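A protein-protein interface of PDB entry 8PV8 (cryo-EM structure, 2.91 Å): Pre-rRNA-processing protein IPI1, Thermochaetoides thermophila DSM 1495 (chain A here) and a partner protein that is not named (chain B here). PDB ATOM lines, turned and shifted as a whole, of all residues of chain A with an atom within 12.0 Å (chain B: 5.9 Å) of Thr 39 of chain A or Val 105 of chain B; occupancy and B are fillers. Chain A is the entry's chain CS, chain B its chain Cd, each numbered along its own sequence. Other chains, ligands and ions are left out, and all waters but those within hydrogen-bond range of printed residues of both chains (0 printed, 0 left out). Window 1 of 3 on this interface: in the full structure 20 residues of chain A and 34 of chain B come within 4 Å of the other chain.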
ATOM      1  N   THR A  35      -1.173  -6.914  -1.159  1.00  0.00           N
ATOM      2  CA  THR A  35      -0.627  -5.851  -1.989  1.00  0.00           C
ATOM      3  C   THR A  35      -1.361  -4.528  -1.827  1.00  0.00           C
ATOM      4  O   THR A  35      -1.008  -3.557  -2.504  1.00  0.00           O
ATOM      5  CB  THR A  35      -0.651  -6.267  -3.461  1.00  0.00           C
ATOM      6  OG1 THR A  35      -1.984  -6.636  -3.834  1.00  0.00           O
ATOM      7  CG2 THR A  35       0.277  -7.442  -3.686  1.00  0.00           C
ATOM      8  N   SER A  36      -2.370  -4.465  -0.963  1.00  0.00           N
ATOM      9  CA  SER A  36      -3.078  -3.213  -0.738  1.00  0.00           C
ATOM     10  C   SER A  36      -2.212  -2.252   0.064  1.00  0.00           C
ATOM     11  O   SER A  36      -1.547  -2.643   1.026  1.00  0.00           O
ATOM     12  CB  SER A  36      -4.395  -3.470  -0.008  1.00  0.00           C
ATOM     13  OG  SER A  36      -4.165  -3.999   1.286  1.00  0.00           O
ATOM     14  N   PHE A  37      -2.221  -0.984  -0.340  1.00  0.00           N
ATOM     15  CA  PHE A  37      -1.430   0.033   0.335  1.00  0.00           C
ATOM     16  C   PHE A  37      -2.160   1.365   0.272  1.00  0.00           C
ATOM     17  O   PHE A  37      -2.979   1.591  -0.624  1.00  0.00           O
ATOM     18  CB  PHE A  37      -0.024   0.150  -0.280  1.00  0.00           C
ATOM     19  CG  PHE A  37      -0.014   0.543  -1.736  1.00  0.00           C
ATOM     20  CD1 PHE A  37       0.080   1.874  -2.115  1.00  0.00           C
ATOM     21  CD2 PHE A  37      -0.077  -0.425  -2.726  1.00  0.00           C
ATOM     22  CE1 PHE A  37       0.095   2.230  -3.447  1.00  0.00           C
ATOM     23  CE2 PHE A  37      -0.063  -0.073  -4.062  1.00  0.00           C
ATOM     24  CZ  PHE A  37       0.024   1.257  -4.421  1.00  0.00           C
ATOM     25  N   LYS A  38      -1.856   2.236   1.226  1.00  0.00           N
ATOM     26  CA  LYS A  38      -2.399   3.583   1.277  1.00  0.00           C
ATOM     27  C   LYS A  38      -1.262   4.592   1.204  1.00  0.00           C
ATOM     28  O   LYS A  38      -0.167   4.355   1.725  1.00  0.00           O
ATOM     29  CB  LYS A  38      -3.210   3.806   2.556  1.00  0.00           C
ATOM     30  CG  LYS A  38      -4.461   2.958   2.674  1.00  0.00           C
ATOM     31  CD  LYS A  38      -5.183   3.252   3.979  1.00  0.00           C
ATOM     32  CE  LYS A  38      -6.410   2.374   4.147  1.00  0.00           C
ATOM     33  NZ  LYS A  38      -7.099   2.637   5.440  1.00  0.00           N
ATOM     34  N   THR A  39      -1.525   5.721   0.552  1.00  0.00           N
ATOM     35  CA  THR A  39      -0.513   6.743   0.337  1.00  0.00           C
ATOM     36  C   THR A  39      -1.009   8.090   0.842  1.00  0.00           C
ATOM     37  O   THR A  39      -2.198   8.406   0.757  1.00  0.00           O
ATOM     38  CB  THR A  39      -0.135   6.860  -1.144  1.00  0.00           C
ATOM     39  OG1 THR A  39      -1.324   6.977  -1.936  1.00  0.00           O
ATOM     40  CG2 THR A  39       0.645   5.639  -1.589  1.00  0.00           C
ATOM     41  N   LYS A  40      -0.076   8.880   1.366  1.00  0.00           N
ATOM     42  CA  LYS A  40      -0.352  10.228   1.835  1.00  0.00           C
ATOM     43  C   LYS A  40       0.576  11.198   1.117  1.00  0.00           C
ATOM     44  O   LYS A  40       1.731  10.874   0.827  1.00  0.00           O
ATOM     45  CB  LYS A  40      -0.177  10.339   3.357  1.00  0.00           C
ATOM     46  CG  LYS A  40      -0.772  11.599   3.969  1.00  0.00           C
ATOM     47  CD  LYS A  40      -0.587  11.628   5.478  1.00  0.00           C
ATOM     48  CE  LYS A  40      -1.205  10.405   6.136  1.00  0.00           C
ATOM     49  NZ  LYS A  40      -1.030  10.423   7.615  1.00  0.00           N
ATOM     50  N   SER A  41       0.062  12.389   0.831  1.00  0.00           N
ATOM     51  CA  SER A  41       0.768  13.381   0.032  1.00  0.00           C
ATOM     52  C   SER A  41       1.473  14.379   0.939  1.00  0.00           C
ATOM     53  O   SER A  41       0.854  14.954   1.841  1.00  0.00           O
ATOM     54  CB  SER A  41      -0.198  14.112  -0.903  1.00  0.00           C
ATOM     55  OG  SER A  41      -1.174  14.828  -0.166  1.00  0.00           O
ATOM     56  N   ILE A  42       2.769  14.577   0.696  1.00  0.00           N
ATOM     57  CA  ILE A  42       3.534  15.580   1.425  1.00  0.00           C
ATOM     58  C   ILE A  42       3.393  16.928   0.732  1.00  0.00           C
ATOM     59  O   ILE A  42       3.642  17.059  -0.473  1.00  0.00           O
ATOM     60  CB  ILE A  42       5.008  15.154   1.528  1.00  0.00           C
ATOM     61  CG1 ILE A  42       5.153  13.926   2.430  1.00  0.00           C
ATOM     62  CG2 ILE A  42       5.869  16.295   2.035  1.00  0.00           C
ATOM     63  CD1 ILE A  42       4.442  14.052   3.763  1.00  0.00           C
ATOM     64  N   VAL A  43       2.990  17.941   1.495  1.00  0.00           N
ATOM     65  CA  VAL A  43       2.783  19.285   0.971  1.00  0.00           C
ATOM     66  C   VAL A  43       3.634  20.265   1.772  1.00  0.00           C
ATOM     67  O   VAL A  43       3.767  20.140   2.995  1.00  0.00           O
ATOM     68  CB  VAL A  43       1.283  19.673   0.973  1.00  0.00           C
ATOM     69  CG1 VAL A  43       0.705  19.758   2.385  1.00  0.00           C
ATOM     70  CG2 VAL A  43       1.057  20.976   0.216  1.00  0.00           C
ATOM     71  N   VAL A  44       4.269  21.197   1.068  1.00  0.00           N
ATOM     72  CA  VAL A  44       5.072  22.245   1.684  1.00  0.00           C
ATOM     73  C   VAL A  44       4.235  23.515   1.716  1.00  0.00           C
ATOM     74  O   VAL A  44       3.871  24.054   0.665  1.00  0.00           O
ATOM     75  CB  VAL A  44       6.389  22.469   0.925  1.00  0.00           C
ATOM     76  CG1 VAL A  44       7.214  23.546   1.606  1.00  0.00           C
ATOM     77  CG2 VAL A  44       7.172  21.171   0.828  1.00  0.00           C
ATOM     78  N   LYS B  98       3.447   5.137  -8.075  1.00  0.00           N
ATOM     79  CA  LYS B  98       3.667   5.835  -6.811  1.00  0.00           C
ATOM     80  C   LYS B  98       5.052   6.475  -6.741  1.00  0.00           C
ATOM     81  O   LYS B  98       5.180   7.619  -6.288  1.00  0.00           O
ATOM     82  CB  LYS B  98       3.443   4.884  -5.636  1.00  0.00           C
ATOM     83  CG  LYS B  98       2.114   5.106  -4.927  1.00  0.00           C
ATOM     84  CD  LYS B  98       0.936   5.003  -5.886  1.00  0.00           C
ATOM     85  CE  LYS B  98      -0.377   5.345  -5.205  1.00  0.00           C
ATOM     86  NZ  LYS B  98      -1.524   5.263  -6.150  1.00  0.00           N
ATOM     87  N   PRO B 102       7.095  12.295  -6.582  1.00  0.00           N
ATOM     88  CA  PRO B 102       8.013  12.406  -5.441  1.00  0.00           C
ATOM     89  C   PRO B 102       7.403  13.017  -4.190  1.00  0.00           C
ATOM     90  O   PRO B 102       8.066  13.031  -3.148  1.00  0.00           O
ATOM     91  CB  PRO B 102       9.129  13.304  -5.994  1.00  0.00           C
ATOM     92  CG  PRO B 102       8.448  14.149  -7.002  1.00  0.00           C
ATOM     93  CD  PRO B 102       7.414  13.268  -7.642  1.00  0.00           C
ATOM     94  N   TYR B 103       6.171  13.525  -4.254  1.00  0.00           N
ATOM     95  CA  TYR B 103       5.526  14.161  -3.110  1.00  0.00           C
ATOM     96  C   TYR B 103       4.566  13.224  -2.387  1.00  0.00           C
ATOM     97  O   TYR B 103       3.843  13.660  -1.486  1.00  0.00           O
ATOM     98  CB  TYR B 103       4.795  15.431  -3.548  1.00  0.00           C
ATOM     99  CG  TYR B 103       5.702  16.615  -3.793  1.00  0.00           C
ATOM    100  CD1 TYR B 103       6.512  16.678  -4.920  1.00  0.00           C
ATOM    101  CD2 TYR B 103       5.748  17.673  -2.895  1.00  0.00           C
ATOM    102  CE1 TYR B 103       7.340  17.759  -5.144  1.00  0.00           C
ATOM    103  CE2 TYR B 103       6.572  18.757  -3.111  1.00  0.00           C
ATOM    104  CZ  TYR B 103       7.364  18.794  -4.237  1.00  0.00           C
ATOM    105  OH  TYR B 103       8.187  19.872  -4.455  1.00  0.00           O
ATOM    106  N   THR B 104       4.541  11.950  -2.766  1.00  0.00           N
ATOM    107  CA  THR B 104       3.686  10.954  -2.135  1.00  0.00           C
ATOM    108  C   THR B 104       4.560   9.953  -1.396  1.00  0.00           C
ATOM    109  O   THR B 104       5.549   9.461  -1.948  1.00  0.00           O
ATOM    110  CB  THR B 104       2.817  10.232  -3.165  1.00  0.00           C
ATOM    111  OG1 THR B 104       3.621   9.852  -4.287  1.00  0.00           O
ATOM    112  CG2 THR B 104       1.694  11.138  -3.640  1.00  0.00           C
ATOM    113  N   VAL B 105       4.195   9.654  -0.154  1.00  0.00           N
ATOM    114  CA  VAL B 105       4.953   8.747   0.698  1.00  0.00           C
ATOM    115  C   VAL B 105       4.032   7.616   1.133  1.00  0.00           C
ATOM    116  O   VAL B 105       2.824   7.821   1.311  1.00  0.00           O
ATOM    117  CB  VAL B 105       5.563   9.473   1.908  1.00  0.00           C
ATOM    118  CG1 VAL B 105       6.681  10.392   1.455  1.00  0.00           C
ATOM    119  CG2 VAL B 105       4.506  10.277   2.630  1.00  0.00           C
ATOM    120  N   LEU B 106       4.597   6.420   1.273  1.00  0.00           N
ATOM    121  CA  LEU B 106       3.806   5.243   1.602  1.00  0.00           C
ATOM    122  C   LEU B 106       3.450   5.221   3.084  1.00  0.00           C
ATOM    123  O   LEU B 106       4.117   5.839   3.918  1.00  0.00           O
ATOM    124  CB  LEU B 106       4.571   3.966   1.238  1.00  0.00           C
ATOM    125  CG  LEU B 106       4.549   3.404  -0.189  1.00  0.00           C
ATOM    126  CD1 LEU B 106       3.139   2.994  -0.573  1.00  0.00           C
ATOM    127  CD2 LEU B 106       5.146   4.348  -1.230  1.00  0.00           C
ATOM    128  N   LEU B 107       2.383   4.496   3.406  1.00  0.00           N
ATOM    129  CA  LEU B 107       2.023   4.190   4.781  1.00  0.00           C
ATOM    130  C   LEU B 107       2.356   2.738   5.091  1.00  0.00           C
ATOM    131  O   LEU B 107       1.956   1.832   4.352  1.00  0.00           O
ATOM    132  CB  LEU B 107       0.537   4.445   5.042  1.00  0.00           C
ATOM    133  CG  LEU B 107       0.040   5.882   4.920  1.00  0.00           C
ATOM    134  CD1 LEU B 107      -1.470   5.933   4.961  1.00  0.00           C
ATOM    135  CD2 LEU B 107       0.600   6.679   6.067  1.00  0.00           C
ATOM    136  N   HIS B 265      13.362  10.071   3.729  1.00  0.00           N
ATOM    137  CA  HIS B 265      12.756  11.142   2.945  1.00  0.00           C
ATOM    138  C   HIS B 265      13.716  12.316   2.806  1.00  0.00           C
ATOM    139  O   HIS B 265      14.140  12.893   3.808  1.00  0.00           O
ATOM    140  CB  HIS B 265      11.449  11.609   3.583  1.00  0.00           C
ATOM    141  CG  HIS B 265      10.512  10.496   3.927  1.00  0.00           C
ATOM    142  ND1 HIS B 265       9.939   9.686   2.972  1.00  0.00           N
ATOM    143  CD2 HIS B 265      10.046  10.059   5.120  1.00  0.00           C
ATOM    144  CE1 HIS B 265       9.160   8.796   3.562  1.00  0.00           C
ATOM    145  NE2 HIS B 265       9.208   9.002   4.865  1.00  0.00           N
ATOM    146  N   PHE B 317       5.950  14.865   8.673  1.00  0.00           N
ATOM    147  CA  PHE B 317       6.742  13.635   8.663  1.00  0.00           C
ATOM    148  C   PHE B 317       6.613  12.873   9.982  1.00  0.00           C
ATOM    149  O   PHE B 317       6.631  11.634   9.997  1.00  0.00           O
ATOM    150  CB  PHE B 317       8.203  13.947   8.350  1.00  0.00           C
ATOM    151  CG  PHE B 317       8.460  14.218   6.896  1.00  0.00           C
ATOM    152  CD1 PHE B 317       8.129  13.273   5.939  1.00  0.00           C
ATOM    153  CD2 PHE B 317       9.036  15.407   6.485  1.00  0.00           C
ATOM    154  CE1 PHE B 317       8.362  13.512   4.599  1.00  0.00           C
ATOM    155  CE2 PHE B 317       9.273  15.651   5.146  1.00  0.00           C
ATOM    156  CZ  PHE B 317       8.935  14.701   4.202  1.00  0.00           C
ATOM    157  N   LEU B 320       3.406  10.982   9.704  1.00  0.00           N
ATOM    158  CA  LEU B 320       3.682   9.764   8.940  1.00  0.00           C
ATOM    159  C   LEU B 320       4.385   8.686   9.760  1.00  0.00           C
ATOM    160  O   LEU B 320       4.030   7.509   9.639  1.00  0.00           O
ATOM    161  CB  LEU B 320       4.511  10.066   7.686  1.00  0.00           C
ATOM    162  CG  LEU B 320       3.863  10.537   6.377  1.00  0.00           C
ATOM    163  CD1 LEU B 320       2.980   9.425   5.878  1.00  0.00           C
ATOM    164  CD2 LEU B 320       3.043  11.800   6.470  1.00  0.00           C
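The backbone carbonyl oxygen (O) of Tyr 103 of chain B lies within hydrogen-bond range of the backbone NH (N) of Ile 42 of chain A (2.6 Å).
The backbone NH (N) of Val 105 of chain B is in hydrogen-bond range of the backbone carbonyl oxygen (O) of Lys 40 of chain A, 2.9 Å away.
N of Leu 107 of chain B is in hydrogen-bond range of O of Lys 38 of chain A (3.1 Å).
Phe 37 of chain A touches Lys 98 of chain B.
Leu 106 of chain B touches Lys 38 of chain A (C to O, 3.96 Å).
Lys 98 of chain B touches Thr 39 of chain A (CG to CG2, 3.7 Å).
Leu 106 of chain B touches Thr 39 of chain A.
Lys 40 of chain A touches Thr 104 of chain B (O to CA, 3.5 Å).
Leu 320 of chain B touches Lys 40 of chain A.
CA of Ser 41 of chain A touches O of Tyr 103 of chain B, 3.4 Å away.
Ile 42 of chain A touches Val 105 of chain B (CG1 to CG2, 3.7 Å).
Phe 317 of chain B touches Ile 42 of chain A (CE1 to CG1, 3.9 Å).
Leu 320 of chain B touches Ile 42 of chain A (CD2 to CD1, 3.8 Å).
O of Lys 98 of chain B is in hydrogen-bond range of OG1 of Thr 104 of chain B.
Hydrophobic or aromatic side chains of chain B that line the printed part of chain A: Tyr 103, Val 105, Leu 106, Leu 107, Phe 317 and Leu 320.
Hydrophobic or aromatic side chains of chain A within 4 Å of the printed part of chain B: Phe 37 and Ile 42.
Among the printed residues, 15 pairs touch across the chains.
Of the printed residues of chain B, Phe 37 of chain A touches Lys 98 and Leu 106.
Printed residues of chain B within 4 Å of Lys 40 of chain A: Thr 104, Val 105 and Leu 320.
Printed residues of chain B within 4 Å of Ser 41 of chain A: Tyr 103.
Of the printed residues of chain B, Ile 42 of chain A touches Tyr 103, Val 105, Phe 317 and Leu 320.
Lys 98 of chain B touches two residues of chain A.
Val 105 of chain B touches just these residues of chain A: Thr 39, Lys 40 and Ile 42.
Of chain A, only Phe 37 (3.6 Å), Lys 38 (3.96 Å) and Thr 39 (3.8 Å) come within 4 Å of Leu 106 of chain B.
Leu 107 of chain B touches just one residue of chain A: Lys 38.
Printed residues of chain A within 4 Å of Phe 317 of chain B: Ile 42 (3.9 Å).
The nearest residue of chain B that does not touch Thr 39 of chain A is Leu 107 of chain B (4.4 Å).
The nearest printed residue of chain B that does not touch Ile 42 of chain A is Thr 104 of chain B (4.7 Å).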
